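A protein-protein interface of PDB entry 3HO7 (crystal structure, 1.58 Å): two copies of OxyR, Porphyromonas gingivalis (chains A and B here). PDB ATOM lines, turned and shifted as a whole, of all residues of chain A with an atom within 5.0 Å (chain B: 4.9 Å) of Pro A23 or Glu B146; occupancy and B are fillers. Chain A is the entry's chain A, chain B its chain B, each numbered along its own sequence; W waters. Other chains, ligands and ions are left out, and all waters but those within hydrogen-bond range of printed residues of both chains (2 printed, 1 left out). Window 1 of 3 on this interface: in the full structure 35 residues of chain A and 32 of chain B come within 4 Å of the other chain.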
ATOM      1  N   LEU A  18     -23.847   6.527  10.877  1.00  0.00           N
ATOM      2  CA  LEU A  18     -22.655   6.681  10.060  1.00  0.00           C
ATOM      3  C   LEU A  18     -22.010   8.042  10.270  1.00  0.00           C
ATOM      4  O   LEU A  18     -22.696   9.038  10.513  1.00  0.00           O
ATOM      5  CB  LEU A  18     -22.977   6.477   8.581  1.00  0.00           C
ATOM      6  CG  LEU A  18     -23.058   5.017   8.131  1.00  0.00           C
ATOM      7  CD1 LEU A  18     -23.985   4.229   9.039  1.00  0.00           C
ATOM      8  CD2 LEU A  18     -23.498   4.926   6.675  1.00  0.00           C
ATOM      9  N   PRO A  19     -20.676   8.090  10.173  1.00  0.00           N
ATOM     10  CA  PRO A  19     -19.939   9.336  10.316  1.00  0.00           C
ATOM     11  C   PRO A  19     -20.264  10.289   9.178  1.00  0.00           C
ATOM     12  O   PRO A  19     -20.107  11.500   9.322  1.00  0.00           O
ATOM     13  CB  PRO A  19     -18.473   8.897  10.220  1.00  0.00           C
ATOM     14  CG  PRO A  19     -18.481   7.412  10.402  1.00  0.00           C
ATOM     15  CD  PRO A  19     -19.793   6.951   9.880  1.00  0.00           C
ATOM     16  N   THR A  20     -20.703   9.738   8.050  1.00  0.00           N
ATOM     17  CA  THR A  20     -21.062  10.547   6.893  1.00  0.00           C
ATOM     18  C   THR A  20     -22.535  10.954   6.920  1.00  0.00           C
ATOM     19  O   THR A  20     -23.042  11.552   5.966  1.00  0.00           O
ATOM     20  CB  THR A  20     -20.749   9.816   5.571  1.00  0.00           C
ATOM     21  OG1 THR A  20     -21.250   8.473   5.633  1.00  0.00           O
ATOM     22  CG2 THR A  20     -19.244   9.775   5.337  1.00  0.00           C
ATOM     23  N   ILE A  21     -23.214  10.628   8.016  1.00  0.00           N
ATOM     24  CA  ILE A  21     -24.607  11.019   8.211  1.00  0.00           C
ATOM     25  C   ILE A  21     -24.746  11.850   9.484  1.00  0.00           C
ATOM     26  O   ILE A  21     -25.408  12.888   9.495  1.00  0.00           O
ATOM     27  CB  ILE A  21     -25.535   9.787   8.338  1.00  0.00           C
ATOM     28  CG1 ILE A  21     -25.530   8.957   7.052  1.00  0.00           C
ATOM     29  CG2 ILE A  21     -26.958  10.213   8.684  1.00  0.00           C
ATOM     30  CD1 ILE A  21     -26.471   7.773   7.104  1.00  0.00           C
ATOM     31  N   ALA A  22     -24.101  11.389  10.550  1.00  0.00           N
ATOM     32  CA  ALA A  22     -24.263  11.970  11.883  1.00  0.00           C
ATOM     33  C   ALA A  22     -24.292  13.495  11.919  1.00  0.00           C
ATOM     34  O   ALA A  22     -25.189  14.087  12.524  1.00  0.00           O
ATOM     35  CB  ALA A  22     -23.186  11.442  12.818  1.00  0.00           C
ATOM     36  N   PRO A  23     -23.298  14.140  11.290  1.00  0.00           N
ATOM     37  CA  PRO A  23     -23.135  15.591  11.385  1.00  0.00           C
ATOM     38  C   PRO A  23     -24.267  16.355  10.714  1.00  0.00           C
ATOM     39  O   PRO A  23     -24.610  17.460  11.139  1.00  0.00           O
ATOM     40  CB  PRO A  23     -21.823  15.850  10.628  1.00  0.00           C
ATOM     41  CG  PRO A  23     -21.137  14.528  10.556  1.00  0.00           C
ATOM     42  CD  PRO A  23     -22.232  13.516  10.489  1.00  0.00           C
ATOM     43  N   TYR A  24     -24.837  15.754   9.678  1.00  0.00           N
ATOM     44  CA  TYR A  24     -25.828  16.420   8.845  1.00  0.00           C
ATOM     45  C   TYR A  24     -27.250  16.140   9.311  1.00  0.00           C
ATOM     46  O   TYR A  24     -28.107  17.023   9.266  1.00  0.00           O
ATOM     47  CB  TYR A  24     -25.637  15.986   7.391  1.00  0.00           C
ATOM     48  CG  TYR A  24     -24.174  15.848   7.047  1.00  0.00           C
ATOM     49  CD1 TYR A  24     -23.380  16.971   6.874  1.00  0.00           C
ATOM     50  CD2 TYR A  24     -23.579  14.598   6.936  1.00  0.00           C
ATOM     51  CE1 TYR A  24     -22.034  16.856   6.579  1.00  0.00           C
ATOM     52  CE2 TYR A  24     -22.234  14.472   6.641  1.00  0.00           C
ATOM     53  CZ  TYR A  24     -21.467  15.607   6.465  1.00  0.00           C
ATOM     54  OH  TYR A  24     -20.127  15.498   6.172  1.00  0.00           O
ATOM     55  N   LEU A  25     -27.490  14.918   9.774  1.00  0.00           N
ATOM     56  CA  LEU A  25     -28.830  14.504  10.189  1.00  0.00           C
ATOM     57  C   LEU A  25     -29.135  14.816  11.651  1.00  0.00           C
ATOM     58  O   LEU A  25     -30.193  15.357  11.970  1.00  0.00           O
ATOM     59  CB  LEU A  25     -29.037  13.012   9.931  1.00  0.00           C
ATOM     60  CG  LEU A  25     -30.374  12.458  10.428  1.00  0.00           C
ATOM     61  CD1 LEU A  25     -31.528  13.221   9.788  1.00  0.00           C
ATOM     62  CD2 LEU A  25     -30.486  10.968  10.151  1.00  0.00           C
ATOM     63  N   LEU A  26     -28.216  14.463  12.543  1.00  0.00           N
ATOM     64  CA  LEU A  26     -28.485  14.563  13.975  1.00  0.00           C
ATOM     65  C   LEU A  26     -28.828  15.976  14.450  1.00  0.00           C
ATOM     66  O   LEU A  26     -29.727  16.154  15.272  1.00  0.00           O
ATOM     67  CB  LEU A  26     -27.333  13.961  14.786  1.00  0.00           C
ATOM     68  CG  LEU A  26     -27.125  12.469  14.511  1.00  0.00           C
ATOM     69  CD1 LEU A  26     -26.017  11.907  15.386  1.00  0.00           C
ATOM     70  CD2 LEU A  26     -28.420  11.690  14.707  1.00  0.00           C
ATOM     71  N   PRO A  27     -28.115  16.992  13.942  1.00  0.00           N
ATOM     72  CA  PRO A  27     -28.491  18.344  14.332  1.00  0.00           C
ATOM     73  C   PRO A  27     -29.988  18.580  14.135  1.00  0.00           C
ATOM     74  O   PRO A  27     -30.606  19.311  14.908  1.00  0.00           O
ATOM     75  CB  PRO A  27     -27.683  19.215  13.370  1.00  0.00           C
ATOM     76  CG  PRO A  27     -26.461  18.410  13.097  1.00  0.00           C
ATOM     77  CD  PRO A  27     -26.912  16.971  13.092  1.00  0.00           C
ATOM     78  N   MET A 145     -14.754  13.117   6.005  1.00  0.00           N
ATOM     79  CA  MET A 145     -15.370  14.137   5.172  1.00  0.00           C
ATOM     80  C   MET A 145     -14.823  15.506   5.543  1.00  0.00           C
ATOM     81  O   MET A 145     -14.579  16.354   4.674  1.00  0.00           O
ATOM     82  CB  MET A 145     -16.890  14.132   5.355  1.00  0.00           C
ATOM     83  CG  MET A 145     -17.618  15.101   4.437  1.00  0.00           C
ATOM     84  SD  MET A 145     -17.776  14.464   2.758  1.00  0.00           S
ATOM     85  CE  MET A 145     -18.785  13.013   3.045  1.00  0.00           C
ATOM     86  N   GLU A 146     -14.638  15.712   6.844  1.00  0.00           N
ATOM     87  CA  GLU A 146     -14.134  16.969   7.368  1.00  0.00           C
ATOM     88  C   GLU A 146     -12.788  17.264   6.727  1.00  0.00           C
ATOM     89  O   GLU A 146     -12.577  18.331   6.151  1.00  0.00           O
ATOM     90  CB  GLU A 146     -13.982  16.891   8.889  1.00  0.00           C
ATOM     91  CG  GLU A 146     -13.605  18.212   9.538  1.00  0.00           C
ATOM     92  CD  GLU A 146     -13.346  18.091  11.031  1.00  0.00           C
ATOM     93  OE1 GLU A 146     -13.412  16.964  11.566  1.00  0.00           O
ATOM     94  OE2 GLU A 146     -13.071  19.127  11.671  1.00  0.00           O
ATOM     95  N   MET A 149     -13.056  18.013   2.927  1.00  0.00           N
ATOM     96  CA  MET A 149     -13.604  19.332   2.637  1.00  0.00           C
ATOM     97  C   MET A 149     -12.590  20.424   2.956  1.00  0.00           C
ATOM     98  O   MET A 149     -12.464  21.401   2.219  1.00  0.00           O
ATOM     99  CB  MET A 149     -14.907  19.562   3.402  1.00  0.00           C
ATOM    100  CG  MET A 149     -15.982  18.572   3.027  1.00  0.00           C
ATOM    101  SD  MET A 149     -17.514  18.851   3.928  1.00  0.00           S
ATOM    102  CE  MET A 149     -17.949  20.495   3.377  1.00  0.00           C
ATOM    103  N   GLN A 168     -25.558  23.753   5.767  1.00  0.00           N
ATOM    104  CA  GLN A 168     -24.609  24.013   6.843  1.00  0.00           C
ATOM    105  C   GLN A 168     -23.425  24.817   6.323  1.00  0.00           C
ATOM    106  O   GLN A 168     -22.633  25.345   7.105  1.00  0.00           O
ATOM    107  CB  GLN A 168     -24.105  22.701   7.440  1.00  0.00           C
ATOM    108  CG  GLN A 168     -25.180  21.864   8.103  1.00  0.00           C
ATOM    109  CD  GLN A 168     -24.664  20.521   8.572  1.00  0.00           C
ATOM    110  OE1 GLN A 168     -23.736  19.960   7.986  1.00  0.00           O
ATOM    111  NE2 GLN A 168     -25.263  19.995   9.634  1.00  0.00           N
ATOM    112  N   SER B 144     -17.996  12.631  16.165  1.00  0.00           N
ATOM    113  CA  SER B 144     -16.919  13.316  15.461  1.00  0.00           C
ATOM    114  C   SER B 144     -16.898  14.795  15.824  1.00  0.00           C
ATOM    115  O   SER B 144     -17.913  15.357  16.241  1.00  0.00           O
ATOM    116  CB  SER B 144     -17.069  13.151  13.944  1.00  0.00           C
ATOM    117  OG  SER B 144     -18.208  13.842  13.452  1.00  0.00           O
ATOM    118  N   MET B 145     -15.739  15.424  15.663  1.00  0.00           N
ATOM    119  CA  MET B 145     -15.615  16.852  15.906  1.00  0.00           C
ATOM    120  C   MET B 145     -16.621  17.595  15.039  1.00  0.00           C
ATOM    121  O   MET B 145     -17.253  18.554  15.485  1.00  0.00           O
ATOM    122  CB  MET B 145     -14.199  17.336  15.585  1.00  0.00           C
ATOM    123  CG  MET B 145     -14.002  18.831  15.791  1.00  0.00           C
ATOM    124  SD  MET B 145     -13.767  19.280  17.522  1.00  0.00           S
ATOM    125  CE  MET B 145     -12.040  18.863  17.740  1.00  0.00           C
ATOM    126  N   GLU B 146     -16.764  17.135  13.800  1.00  0.00           N
ATOM    127  CA  GLU B 146     -17.668  17.757  12.841  1.00  0.00           C
ATOM    128  C   GLU B 146     -19.113  17.735  13.328  1.00  0.00           C
ATOM    129  O   GLU B 146     -19.837  18.726  13.201  1.00  0.00           O
ATOM    130  CB  GLU B 146     -17.576  17.063  11.479  1.00  0.00           C
ATOM    131  CG  GLU B 146     -18.470  17.697  10.426  1.00  0.00           C
ATOM    132  CD  GLU B 146     -18.458  16.961   9.097  1.00  0.00           C
ATOM    133  OE1 GLU B 146     -18.175  15.744   9.078  1.00  0.00           O
ATOM    134  OE2 GLU B 146     -18.746  17.609   8.069  1.00  0.00           O
ATOM    135  N   ALA B 147     -19.533  16.598  13.875  1.00  0.00           N
ATOM    136  CA  ALA B 147     -20.898  16.448  14.367  1.00  0.00           C
ATOM    137  C   ALA B 147     -21.160  17.395  15.533  1.00  0.00           C
ATOM    138  O   ALA B 147     -22.169  18.104  15.557  1.00  0.00           O
ATOM    139  CB  ALA B 147     -21.160  15.006  14.778  1.00  0.00           C
ATOM    140  N   PHE B 148     -20.246  17.397  16.500  1.00  0.00           N
ATOM    141  CA  PHE B 148     -20.341  18.288  17.653  1.00  0.00           C
ATOM    142  C   PHE B 148     -20.345  19.758  17.237  1.00  0.00           C
ATOM    143  O   PHE B 148     -21.100  20.563  17.779  1.00  0.00           O
ATOM    144  CB  PHE B 148     -19.207  18.022  18.650  1.00  0.00           C
ATOM    145  CG  PHE B 148     -19.328  16.708  19.369  1.00  0.00           C
ATOM    146  CD1 PHE B 148     -20.423  15.889  19.161  1.00  0.00           C
ATOM    147  CD2 PHE B 148     -18.362  16.308  20.276  1.00  0.00           C
ATOM    148  CE1 PHE B 148     -20.541  14.681  19.824  1.00  0.00           C
ATOM    149  CE2 PHE B 148     -18.478  15.100  20.948  1.00  0.00           C
ATOM    150  CZ  PHE B 148     -19.569  14.290  20.721  1.00  0.00           C
ATOM    151  N   MET B 149     -19.505  20.109  16.268  1.00  0.00           N
ATOM    152  CA  MET B 149     -19.471  21.482  15.780  1.00  0.00           C
ATOM    153  C   MET B 149     -20.795  21.876  15.120  1.00  0.00           C
ATOM    154  O   MET B 149     -21.270  22.998  15.297  1.00  0.00           O
ATOM    155  CB  MET B 149     -18.287  21.703  14.829  1.00  0.00           C
ATOM    156  CG  MET B 149     -16.943  21.818  15.543  1.00  0.00           C
ATOM    157  SD  MET B 149     -15.567  22.212  14.442  1.00  0.00           S
ATOM    158  CE  MET B 149     -16.247  23.608  13.555  1.00  0.00           C
ATOM    159  N   ARG B 150     -21.394  20.952  14.375  1.00  0.00           N
ATOM    160  CA  ARG B 150     -22.681  21.213  13.742  1.00  0.00           C
ATOM    161  C   ARG B 150     -23.762  21.362  14.804  1.00  0.00           C
ATOM    162  O   ARG B 150     -24.602  22.255  14.721  1.00  0.00           O
ATOM    163  CB  ARG B 150     -23.047  20.099  12.761  1.00  0.00           C
ATOM    164  CG  ARG B 150     -22.172  20.050  11.518  1.00  0.00           C
ATOM    165  CD  ARG B 150     -22.195  21.367  10.759  1.00  0.00           C
ATOM    166  NE  ARG B 150     -21.206  22.313  11.265  1.00  0.00           N
ATOM    167  CZ  ARG B 150     -19.898  22.200  11.055  1.00  0.00           C
ATOM    168  NH1 ARG B 150     -19.427  21.173  10.361  1.00  0.00           N
ATOM    169  NH2 ARG B 150     -19.058  23.104  11.545  1.00  0.00           N
HETATM  170  O   HOH W   1     -16.037  14.183   9.437  1.00  0.00           O
HETATM  171  O   HOH W   2     -18.930  11.970  11.828  1.00  0.00           O
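OE2 of Glu B146 is in hydrogen-bond range of OH of Tyr A24 (3.2 Å).
The side-chain amide nitrogen (NE2) of Gln A168 is in hydrogen-bond range of the backbone carbonyl oxygen (O) of Pro A23 (3.0 Å). The side-chain hydroxyl of Ser B144 sits at hydrogen-bond distance from the backbone NH of Ala B147 (3.1 Å).
Among the printed residues, merely in contact across the chains: Pro A23 with Glu B146, Pro A23 with Ala B147, Pro A23 with Arg B150, Pro A27 with Arg B150 and Gln A168 with Arg B150.
Pro A23 touches just these residues of chain B: Glu B146 (3.5 Å), Ala B147 (3.8 Å) and Arg B150 (3.5 Å). Glu B146 touches just these residues of chain A: Pro A23 (3.5 Å) and Tyr A24 (3.2 Å). Printed residues of chain B within 4 Å of Pro A27: Arg B150. Of the printed residues of chain A, Ala B147 touches Pro A23 (3.8 Å). Phe B148 touches none of the printed residues of chain A. The nearest printed residue of chain B that does not touch Tyr A24 is Arg B150 (5.4 Å).
Of the 14 printed residues of chain A, 4 touch a printed residue of chain B. Hydrophobic or aromatic side chains of chain A within 4 Å of the printed part of chain B: Pro A23, Tyr A24 and Pro A27. Of the 7 printed residues of chain B, 3 touch a printed residue of chain A. Among the printed residues, 6 pairs touch across the chains.
Positions printed for both chains: 145, 146 and 149. Of the 6 pairs that touch across the chains among the printed residues, none has its exchanged pair printed and touching as well.
Water W2 bridges the side-chain hydroxyl of Ser B144 (2.6 Å) and the backbone carbonyl oxygen of Pro A19 (2.8 Å). Water W1 lies within hydrogen-bond range of OE1 of Glu B146 (2.7 Å) and N of Glu A146 (3.3 Å).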
